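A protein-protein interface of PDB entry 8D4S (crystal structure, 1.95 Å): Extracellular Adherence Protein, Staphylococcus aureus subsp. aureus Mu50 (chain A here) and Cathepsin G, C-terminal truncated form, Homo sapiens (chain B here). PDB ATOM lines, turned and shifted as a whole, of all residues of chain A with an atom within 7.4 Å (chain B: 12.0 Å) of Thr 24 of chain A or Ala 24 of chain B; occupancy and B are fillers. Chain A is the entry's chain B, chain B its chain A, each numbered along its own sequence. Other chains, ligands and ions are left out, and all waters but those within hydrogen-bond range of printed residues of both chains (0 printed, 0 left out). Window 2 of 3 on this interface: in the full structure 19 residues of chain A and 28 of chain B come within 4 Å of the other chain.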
ATOM      1  N   SER A   2      -3.945  24.768   1.691  1.00  0.00           N
ATOM      2  CA  SER A   2      -4.963  24.822   0.642  1.00  0.00           C
ATOM      3  C   SER A   2      -5.248  23.456   0.025  1.00  0.00           C
ATOM      4  O   SER A   2      -6.009  23.355  -0.934  1.00  0.00           O
ATOM      5  CB  SER A   2      -4.537  25.768  -0.471  1.00  0.00           C
ATOM      6  OG  SER A   2      -3.496  25.168  -1.227  1.00  0.00           O
ATOM      7  N   THR A   3      -4.614  22.413   0.547  1.00  0.00           N
ATOM      8  CA  THR A   3      -4.798  21.065   0.034  1.00  0.00           C
ATOM      9  C   THR A   3      -5.264  20.134   1.144  1.00  0.00           C
ATOM     10  O   THR A   3      -5.134  20.430   2.335  1.00  0.00           O
ATOM     11  CB  THR A   3      -3.513  20.506  -0.587  1.00  0.00           C
ATOM     12  OG1 THR A   3      -2.481  20.478   0.406  1.00  0.00           O
ATOM     13  CG2 THR A   3      -3.072  21.355  -1.772  1.00  0.00           C
ATOM     14  N   ILE A   4      -5.818  18.996   0.722  1.00  0.00           N
ATOM     15  CA  ILE A   4      -6.307  17.954   1.610  1.00  0.00           C
ATOM     16  C   ILE A   4      -5.758  16.628   1.109  1.00  0.00           C
ATOM     17  O   ILE A   4      -5.409  16.477  -0.063  1.00  0.00           O
ATOM     18  CB  ILE A   4      -7.854  17.893   1.673  1.00  0.00           C
ATOM     19  CG1 ILE A   4      -8.441  17.894   0.258  1.00  0.00           C
ATOM     20  CG2 ILE A   4      -8.422  19.054   2.488  1.00  0.00           C
ATOM     21  CD1 ILE A   4      -9.950  17.721   0.218  1.00  0.00           C
ATOM     22  N   GLN A   5      -5.689  15.665   2.018  1.00  0.00           N
ATOM     23  CA  GLN A   5      -5.347  14.289   1.683  1.00  0.00           C
ATOM     24  C   GLN A   5      -6.606  13.430   1.711  1.00  0.00           C
ATOM     25  O   GLN A   5      -7.310  13.391   2.723  1.00  0.00           O
ATOM     26  CB  GLN A   5      -4.302  13.754   2.662  1.00  0.00           C
ATOM     27  CG  GLN A   5      -2.939  14.461   2.538  1.00  0.00           C
ATOM     28  CD  GLN A   5      -2.278  14.200   1.191  1.00  0.00           C
ATOM     29  OE1 GLN A   5      -2.187  13.060   0.747  1.00  0.00           O
ATOM     30  NE2 GLN A   5      -1.825  15.260   0.530  1.00  0.00           N
ATOM     31  N   ILE A   6      -6.889  12.745   0.611  1.00  0.00           N
ATOM     32  CA  ILE A   6      -8.044  11.857   0.512  1.00  0.00           C
ATOM     33  C   ILE A   6      -7.544  10.408   0.490  1.00  0.00           C
ATOM     34  O   ILE A   6      -6.824  10.021  -0.439  1.00  0.00           O
ATOM     35  CB  ILE A   6      -8.893  12.182  -0.725  1.00  0.00           C
ATOM     36  CG1 ILE A   6      -9.671  13.484  -0.457  1.00  0.00           C
ATOM     37  CG2 ILE A   6      -9.815  11.023  -1.084  1.00  0.00           C
ATOM     38  CD1 ILE A   6     -10.385  14.038  -1.640  1.00  0.00           C
ATOM     39  N   TYR A   8      -7.081   6.437  -0.074  1.00  0.00           N
ATOM     40  CA  TYR A   8      -7.494   5.520  -1.123  1.00  0.00           C
ATOM     41  C   TYR A   8      -6.994   4.129  -0.771  1.00  0.00           C
ATOM     42  O   TYR A   8      -6.033   3.969  -0.021  1.00  0.00           O
ATOM     43  CB  TYR A   8      -6.991   5.957  -2.515  1.00  0.00           C
ATOM     44  CG  TYR A   8      -5.497   5.892  -2.727  1.00  0.00           C
ATOM     45  CD1 TYR A   8      -4.882   4.716  -3.181  1.00  0.00           C
ATOM     46  CD2 TYR A   8      -4.699   7.001  -2.498  1.00  0.00           C
ATOM     47  CE1 TYR A   8      -3.505   4.652  -3.363  1.00  0.00           C
ATOM     48  CE2 TYR A   8      -3.321   6.950  -2.683  1.00  0.00           C
ATOM     49  CZ  TYR A   8      -2.733   5.779  -3.120  1.00  0.00           C
ATOM     50  OH  TYR A   8      -1.373   5.742  -3.308  1.00  0.00           O
ATOM     51  N   SER A  22      -2.751   8.145   0.592  1.00  0.00           N
ATOM     52  CA  SER A  22      -3.604   9.306   0.383  1.00  0.00           C
ATOM     53  C   SER A  22      -3.274   9.969  -0.944  1.00  0.00           C
ATOM     54  O   SER A  22      -2.131   9.920  -1.416  1.00  0.00           O
ATOM     55  CB  SER A  22      -3.431  10.335   1.521  1.00  0.00           C
ATOM     56  OG  SER A  22      -4.279  10.032   2.604  1.00  0.00           O
ATOM     57  N   LEU A  23      -4.293  10.592  -1.535  1.00  0.00           N
ATOM     58  CA  LEU A  23      -4.167  11.451  -2.705  1.00  0.00           C
ATOM     59  C   LEU A  23      -4.287  12.911  -2.290  1.00  0.00           C
ATOM     60  O   LEU A  23      -5.142  13.260  -1.471  1.00  0.00           O
ATOM     61  CB  LEU A  23      -5.251  11.136  -3.736  1.00  0.00           C
ATOM     62  CG  LEU A  23      -5.105   9.875  -4.581  1.00  0.00           C
ATOM     63  CD1 LEU A  23      -6.362   9.641  -5.390  1.00  0.00           C
ATOM     64  CD2 LEU A  23      -3.932  10.066  -5.490  1.00  0.00           C
ATOM     65  N   THR A  24      -3.446  13.764  -2.871  1.00  0.00           N
ATOM     66  CA  THR A  24      -3.489  15.201  -2.620  1.00  0.00           C
ATOM     67  C   THR A  24      -4.506  15.875  -3.537  1.00  0.00           C
ATOM     68  O   THR A  24      -4.433  15.731  -4.760  1.00  0.00           O
ATOM     69  CB  THR A  24      -2.108  15.828  -2.842  1.00  0.00           C
ATOM     70  OG1 THR A  24      -1.182  15.304  -1.885  1.00  0.00           O
ATOM     71  CG2 THR A  24      -2.175  17.357  -2.711  1.00  0.00           C
ATOM     72  N   PHE A  25      -5.444  16.615  -2.942  1.00  0.00           N
ATOM     73  CA  PHE A  25      -6.391  17.448  -3.679  1.00  0.00           C
ATOM     74  C   PHE A  25      -6.404  18.850  -3.088  1.00  0.00           C
ATOM     75  O   PHE A  25      -6.063  19.054  -1.924  1.00  0.00           O
ATOM     76  CB  PHE A  25      -7.825  16.901  -3.623  1.00  0.00           C
ATOM     77  CG  PHE A  25      -8.036  15.646  -4.398  1.00  0.00           C
ATOM     78  CD1 PHE A  25      -7.824  14.414  -3.809  1.00  0.00           C
ATOM     79  CD2 PHE A  25      -8.489  15.690  -5.706  1.00  0.00           C
ATOM     80  CE1 PHE A  25      -8.039  13.235  -4.513  1.00  0.00           C
ATOM     81  CE2 PHE A  25      -8.708  14.523  -6.416  1.00  0.00           C
ATOM     82  CZ  PHE A  25      -8.477  13.289  -5.816  1.00  0.00           C
ATOM     83  N   ASN A  26      -6.838  19.819  -3.889  1.00  0.00           N
ATOM     84  CA  ASN A  26      -7.050  21.157  -3.366  1.00  0.00           C
ATOM     85  C   ASN A  26      -8.382  21.224  -2.625  1.00  0.00           C
ATOM     86  O   ASN A  26      -9.354  20.562  -3.000  1.00  0.00           O
ATOM     87  CB  ASN A  26      -7.005  22.180  -4.497  1.00  0.00           C
ATOM     88  CG  ASN A  26      -5.727  22.082  -5.309  1.00  0.00           C
ATOM     89  OD1 ASN A  26      -4.634  22.276  -4.783  1.00  0.00           O
ATOM     90  ND2 ASN A  26      -5.857  21.772  -6.595  1.00  0.00           N
ATOM     91  N   ASN A  38      -7.288  10.163 -13.669  1.00  0.00           N
ATOM     92  CA  ASN A  38      -5.849  10.328 -13.867  1.00  0.00           C
ATOM     93  C   ASN A  38      -5.072  10.165 -12.563  1.00  0.00           C
ATOM     94  O   ASN A  38      -3.924   9.709 -12.583  1.00  0.00           O
ATOM     95  CB  ASN A  38      -5.550  11.688 -14.488  1.00  0.00           C
ATOM     96  CG  ASN A  38      -5.948  11.758 -15.953  1.00  0.00           C
ATOM     97  OD1 ASN A  38      -6.187  10.735 -16.596  1.00  0.00           O
ATOM     98  ND2 ASN A  38      -6.001  12.969 -16.491  1.00  0.00           N
ATOM     99  N   LYS A  39      -5.665  10.538 -11.428  1.00  0.00           N
ATOM    100  CA  LYS A  39      -5.005  10.292 -10.150  1.00  0.00           C
ATOM    101  C   LYS A  39      -5.124   8.835  -9.732  1.00  0.00           C
ATOM    102  O   LYS A  39      -4.197   8.289  -9.120  1.00  0.00           O
ATOM    103  CB  LYS A  39      -5.583  11.204  -9.065  1.00  0.00           C
ATOM    104  CG  LYS A  39      -5.265  12.685  -9.258  1.00  0.00           C
ATOM    105  CD  LYS A  39      -5.773  13.507  -8.072  1.00  0.00           C
ATOM    106  CE  LYS A  39      -5.521  14.999  -8.253  1.00  0.00           C
ATOM    107  NZ  LYS A  39      -4.069  15.312  -8.366  1.00  0.00           N
ATOM    108  N   SER A  42      -2.724   6.889 -11.687  1.00  0.00           N
ATOM    109  CA  SER A  42      -1.380   7.218 -11.225  1.00  0.00           C
ATOM    110  C   SER A  42      -0.981   6.349 -10.035  1.00  0.00           C
ATOM    111  O   SER A  42       0.103   5.748 -10.024  1.00  0.00           O
ATOM    112  CB  SER A  42      -1.307   8.705 -10.869  1.00  0.00           C
ATOM    113  OG  SER A  42       0.019   9.112 -10.572  1.00  0.00           O
ATOM    114  N   VAL A  43      -1.848   6.258  -9.026  1.00  0.00           N
ATOM    115  CA  VAL A  43      -1.525   5.436  -7.864  1.00  0.00           C
ATOM    116  C   VAL A  43      -1.682   3.943  -8.146  1.00  0.00           C
ATOM    117  O   VAL A  43      -1.029   3.128  -7.484  1.00  0.00           O
ATOM    118  CB  VAL A  43      -2.378   5.855  -6.659  1.00  0.00           C
ATOM    119  CG1 VAL A  43      -2.002   7.282  -6.222  1.00  0.00           C
ATOM    120  CG2 VAL A  43      -3.861   5.739  -6.988  1.00  0.00           C
ATOM    121  N   PHE A  46       1.819   3.311  -9.645  1.00  0.00           N
ATOM    122  CA  PHE A  46       2.874   3.390  -8.639  1.00  0.00           C
ATOM    123  C   PHE A  46       2.810   2.215  -7.672  1.00  0.00           C
ATOM    124  O   PHE A  46       3.842   1.630  -7.332  1.00  0.00           O
ATOM    125  CB  PHE A  46       2.782   4.713  -7.870  1.00  0.00           C
ATOM    126  CG  PHE A  46       3.928   4.943  -6.905  1.00  0.00           C
ATOM    127  CD1 PHE A  46       5.192   5.287  -7.372  1.00  0.00           C
ATOM    128  CD2 PHE A  46       3.738   4.821  -5.538  1.00  0.00           C
ATOM    129  CE1 PHE A  46       6.247   5.502  -6.491  1.00  0.00           C
ATOM    130  CE2 PHE A  46       4.791   5.032  -4.648  1.00  0.00           C
ATOM    131  CZ  PHE A  46       6.046   5.377  -5.128  1.00  0.00           C
ATOM    132  N   ILE B  20       6.042   8.550   3.643  1.00  0.00           N
ATOM    133  CA  ILE B  20       6.521   8.186   2.315  1.00  0.00           C
ATOM    134  C   ILE B  20       5.902   9.117   1.295  1.00  0.00           C
ATOM    135  O   ILE B  20       4.679   9.308   1.286  1.00  0.00           O
ATOM    136  CB  ILE B  20       6.168   6.725   1.983  1.00  0.00           C
ATOM    137  CG1 ILE B  20       6.759   5.801   3.045  1.00  0.00           C
ATOM    138  CG2 ILE B  20       6.634   6.362   0.565  1.00  0.00           C
ATOM    139  CD1 ILE B  20       5.860   4.597   3.369  1.00  0.00           C
ATOM    140  N   GLN B  21       6.736   9.696   0.432  1.00  0.00           N
ATOM    141  CA  GLN B  21       6.254  10.498  -0.682  1.00  0.00           C
ATOM    142  C   GLN B  21       5.932   9.580  -1.858  1.00  0.00           C
ATOM    143  O   GLN B  21       6.768   8.764  -2.267  1.00  0.00           O
ATOM    144  CB  GLN B  21       7.282  11.553  -1.085  1.00  0.00           C
ATOM    145  CG  GLN B  21       6.800  12.492  -2.188  1.00  0.00           C
ATOM    146  CD  GLN B  21       7.892  13.437  -2.658  1.00  0.00           C
ATOM    147  OE1 GLN B  21       9.001  13.440  -2.118  1.00  0.00           O
ATOM    148  NE2 GLN B  21       7.584  14.245  -3.665  1.00  0.00           N
ATOM    149  N   SER B  22       4.728   9.712  -2.395  1.00  0.00           N
ATOM    150  CA  SER B  22       4.225   8.797  -3.420  1.00  0.00           C
ATOM    151  C   SER B  22       3.350   9.588  -4.370  1.00  0.00           C
ATOM    152  O   SER B  22       2.193   9.901  -4.036  1.00  0.00           O
ATOM    153  CB  SER B  22       3.435   7.651  -2.798  1.00  0.00           C
ATOM    154  OG  SER B  22       2.140   8.095  -2.423  1.00  0.00           O
ATOM    155  N   PRO B  23       3.843   9.916  -5.560  1.00  0.00           N
ATOM    156  CA  PRO B  23       3.009  10.644  -6.525  1.00  0.00           C
ATOM    157  C   PRO B  23       1.738   9.860  -6.828  1.00  0.00           C
ATOM    158  O   PRO B  23       1.790   8.683  -7.195  1.00  0.00           O
ATOM    159  CB  PRO B  23       3.913  10.765  -7.755  1.00  0.00           C
ATOM    160  CG  PRO B  23       4.866   9.603  -7.630  1.00  0.00           C
ATOM    161  CD  PRO B  23       5.108   9.446  -6.154  1.00  0.00           C
ATOM    162  N   ALA B  24       0.587  10.516  -6.661  1.00  0.00           N
ATOM    163  CA  ALA B  24       0.508  11.942  -6.347  1.00  0.00           C
ATOM    164  C   ALA B  24      -0.119  12.214  -4.973  1.00  0.00           C
ATOM    165  O   ALA B  24      -1.225  12.759  -4.869  1.00  0.00           O
ATOM    166  CB  ALA B  24      -0.280  12.667  -7.432  1.00  0.00           C
ATOM    167  N   GLY B  25       0.609  11.843  -3.923  1.00  0.00           N
ATOM    168  CA  GLY B  25       0.158  12.016  -2.555  1.00  0.00           C
ATOM    169  C   GLY B  25       1.156  11.454  -1.560  1.00  0.00           C
ATOM    170  O   GLY B  25       2.365  11.478  -1.805  1.00  0.00           O
ATOM    171  N   GLN B  26       0.679  10.931  -0.441  1.00  0.00           N
ATOM    172  CA  GLN B  26       1.567  10.472   0.609  1.00  0.00           C
ATOM    173  C   GLN B  26       1.104   9.108   1.099  1.00  0.00           C
ATOM    174  O   GLN B  26      -0.050   8.714   0.910  1.00  0.00           O
ATOM    175  CB  GLN B  26       1.614  11.478   1.769  1.00  0.00           C
ATOM    176  CG  GLN B  26       0.318  11.546   2.545  1.00  0.00           C
ATOM    177  CD  GLN B  26       0.329  12.616   3.611  1.00  0.00           C
ATOM    178  OE1 GLN B  26       1.118  13.556   3.552  1.00  0.00           O
ATOM    179  NE2 GLN B  26      -0.548  12.475   4.601  1.00  0.00           N
ATOM    180  N   SER B  27       2.025   8.380   1.723  1.00  0.00           N
ATOM    181  CA  SER B  27       1.710   7.087   2.297  1.00  0.00           C
ATOM    182  C   SER B  27       2.354   6.989   3.668  1.00  0.00           C
ATOM    183  O   SER B  27       3.336   7.679   3.968  1.00  0.00           O
ATOM    184  CB  SER B  27       2.179   5.941   1.390  1.00  0.00           C
ATOM    185  OG  SER B  27       1.467   5.965   0.163  1.00  0.00           O
ATOM    186  N   ARG B  28       1.772   6.122   4.497  1.00  0.00           N
ATOM    187  CA  ARG B  28       2.271   5.822   5.836  1.00  0.00           C
ATOM    188  C   ARG B  28       2.371   4.310   6.006  1.00  0.00           C
ATOM    189  O   ARG B  28       1.453   3.574   5.631  1.00  0.00           O
ATOM    190  CB  ARG B  28       1.362   6.405   6.922  1.00  0.00           C
ATOM    191  CG  ARG B  28       1.066   7.897   6.775  1.00  0.00           C
ATOM    192  CD  ARG B  28       2.304   8.716   7.087  1.00  0.00           C
ATOM    193  NE  ARG B  28       2.011  10.149   7.168  1.00  0.00           N
ATOM    194  CZ  ARG B  28       2.338  11.038   6.233  1.00  0.00           C
ATOM    195  NH1 ARG B  28       2.975  10.648   5.133  1.00  0.00           N
ATOM    196  NH2 ARG B  28       2.030  12.320   6.400  1.00  0.00           N
ATOM    197  N   TRP B  46       7.925   1.563  -0.517  1.00  0.00           N
ATOM    198  CA  TRP B  46       9.020   2.310  -1.121  1.00  0.00           C
ATOM    199  C   TRP B  46       8.555   3.679  -1.616  1.00  0.00           C
ATOM    200  O   TRP B  46       7.399   3.869  -2.004  1.00  0.00           O
ATOM    201  CB  TRP B  46       9.614   1.518  -2.290  1.00  0.00           C
ATOM    202  CG  TRP B  46      10.749   2.209  -3.002  1.00  0.00           C
ATOM    203  CD1 TRP B  46      12.075   2.107  -2.706  1.00  0.00           C
ATOM    204  CD2 TRP B  46      10.659   3.097  -4.130  1.00  0.00           C
ATOM    205  NE1 TRP B  46      12.814   2.870  -3.574  1.00  0.00           N
ATOM    206  CE2 TRP B  46      11.972   3.489  -4.457  1.00  0.00           C
ATOM    207  CE3 TRP B  46       9.597   3.590  -4.902  1.00  0.00           C
ATOM    208  CZ2 TRP B  46      12.255   4.356  -5.512  1.00  0.00           C
ATOM    209  CZ3 TRP B  46       9.881   4.452  -5.954  1.00  0.00           C
ATOM    210  CH2 TRP B  46      11.198   4.824  -6.248  1.00  0.00           C
ATOM    211  N   GLY B  47       9.484   4.634  -1.624  1.00  0.00           N
ATOM    212  CA  GLY B  47       9.242   5.929  -2.236  1.00  0.00           C
ATOM    213  C   GLY B  47      10.570   6.617  -2.432  1.00  0.00           C
ATOM    214  O   GLY B  47      11.590   6.218  -1.863  1.00  0.00           O
ATOM    215  N   SER B  48      10.543   7.661  -3.258  1.00  0.00           N
ATOM    216  CA  SER B  48      11.741   8.451  -3.518  1.00  0.00           C
ATOM    217  C   SER B  48      12.199   9.225  -2.290  1.00  0.00           C
ATOM    218  O   SER B  48      13.361   9.639  -2.225  1.00  0.00           O
ATOM    219  CB  SER B  48      11.478   9.433  -4.658  1.00  0.00           C
ATOM    220  OG  SER B  48      10.472  10.359  -4.272  1.00  0.00           O
ATOM    221  N   ASN B  49      11.311   9.425  -1.323  1.00  0.00           N
ATOM    222  CA  ASN B  49      11.587  10.258  -0.162  1.00  0.00           C
ATOM    223  C   ASN B  49      10.871   9.628   1.022  1.00  0.00           C
ATOM    224  O   ASN B  49       9.642   9.534   1.005  1.00  0.00           O
ATOM    225  CB  ASN B  49      11.096  11.685  -0.417  1.00  0.00           C
ATOM    226  CG  ASN B  49      11.722  12.688   0.501  1.00  0.00           C
ATOM    227  OD1 ASN B  49      11.748  12.503   1.717  1.00  0.00           O
ATOM    228  ND2 ASN B  49      12.243  13.766  -0.074  1.00  0.00           N
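Among the printed residues, merely in contact across the chains: Ser 22 of chain A with Gly 25 of chain B (3.3 Å), Gln 5 of chain A with Gln 26 of chain B (3.4 Å), Phe 46 of chain A with Ser 22 of chain B (3.5 Å), Thr 24 of chain A with Gly 25 of chain B (3.6 Å), Phe 46 of chain A with Trp 46 of chain B (3.7 Å), Ser 42 of chain A with Pro 23 of chain B (3.8 Å) and Leu 23 of chain A with Ala 24 of chain B (3.9 Å).
N of Ile 6 of chain A is in hydrogen-bond range of O of Leu 23 of chain A (2.8 Å). The guanidinium group of Arg 28 of chain B lies close to the side-chain amide nitrogen of Gln 26 of chain B (3.1 Å). The side-chain hydroxyl of Ser 22 of chain B lies within hydrogen-bond range of the side-chain hydroxyl of Ser 27 of chain B (3.4 Å). The backbone carbonyl oxygen (O) of Gly 25 of chain B lies close to the side-chain hydroxyl (OG) of Ser 22 of chain B. NE2 of Gln 5 of chain A lies within hydrogen-bond range of OG1 of Thr 24 of chain A (2.5 Å).
No residue of chain B comes within 4 Å of Thr 3 of chain A. No residue of chain B comes within 4 Å of Ile 4 of chain A. No residue of chain B comes within 4 Å of Ile 6 of chain A. Ser 22 of chain A touches two residues of chain B. Of chain B, only Ala 24 (3.2 Å) and Gly 25 (3.6 Å) come within 4 Å of Thr 24 of chain A. No residue of chain B comes within 4 Å of Asn 26 of chain A. No residue of chain B comes within 4 Å of Lys 39 of chain A. No residue of chain B comes within 4 Å of Val 43 of chain A. Of the printed residues of chain B, Phe 46 of chain A touches Ser 22 (3.5 Å) and Trp 46 (3.7 Å). Of chain A, only Leu 23 (3.9 Å) and Thr 24 (3.2 Å) come within 4 Å of Ala 24 of chain B. Printed residues of chain A within 4 Å of Gln 26 of chain B: Gln 5 (3.4 Å) and Ser 22 (2.8 Å). Ser 48 of chain B touches none of the printed residues of chain A. The nearest residue of chain B that does not touch Thr 24 of chain A is Gln 26 of chain B (5.0 Å).
Hydrophobic or aromatic side chains of chain A that line the printed part of chain B: Leu 23 and Phe 46. Of the 13 printed residues of chain B, 6 touch a printed residue of chain A. Hydrophobic or aromatic side chains of chain B that line the printed part of chain A: Trp 46.
O of Ala 24 of chain B is in hydrogen-bond range of N of Thr 24 of chain A. N of Ser 22 of chain A sits at hydrogen-bond distance from O of Gln 26 of chain B (2.8 Å).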
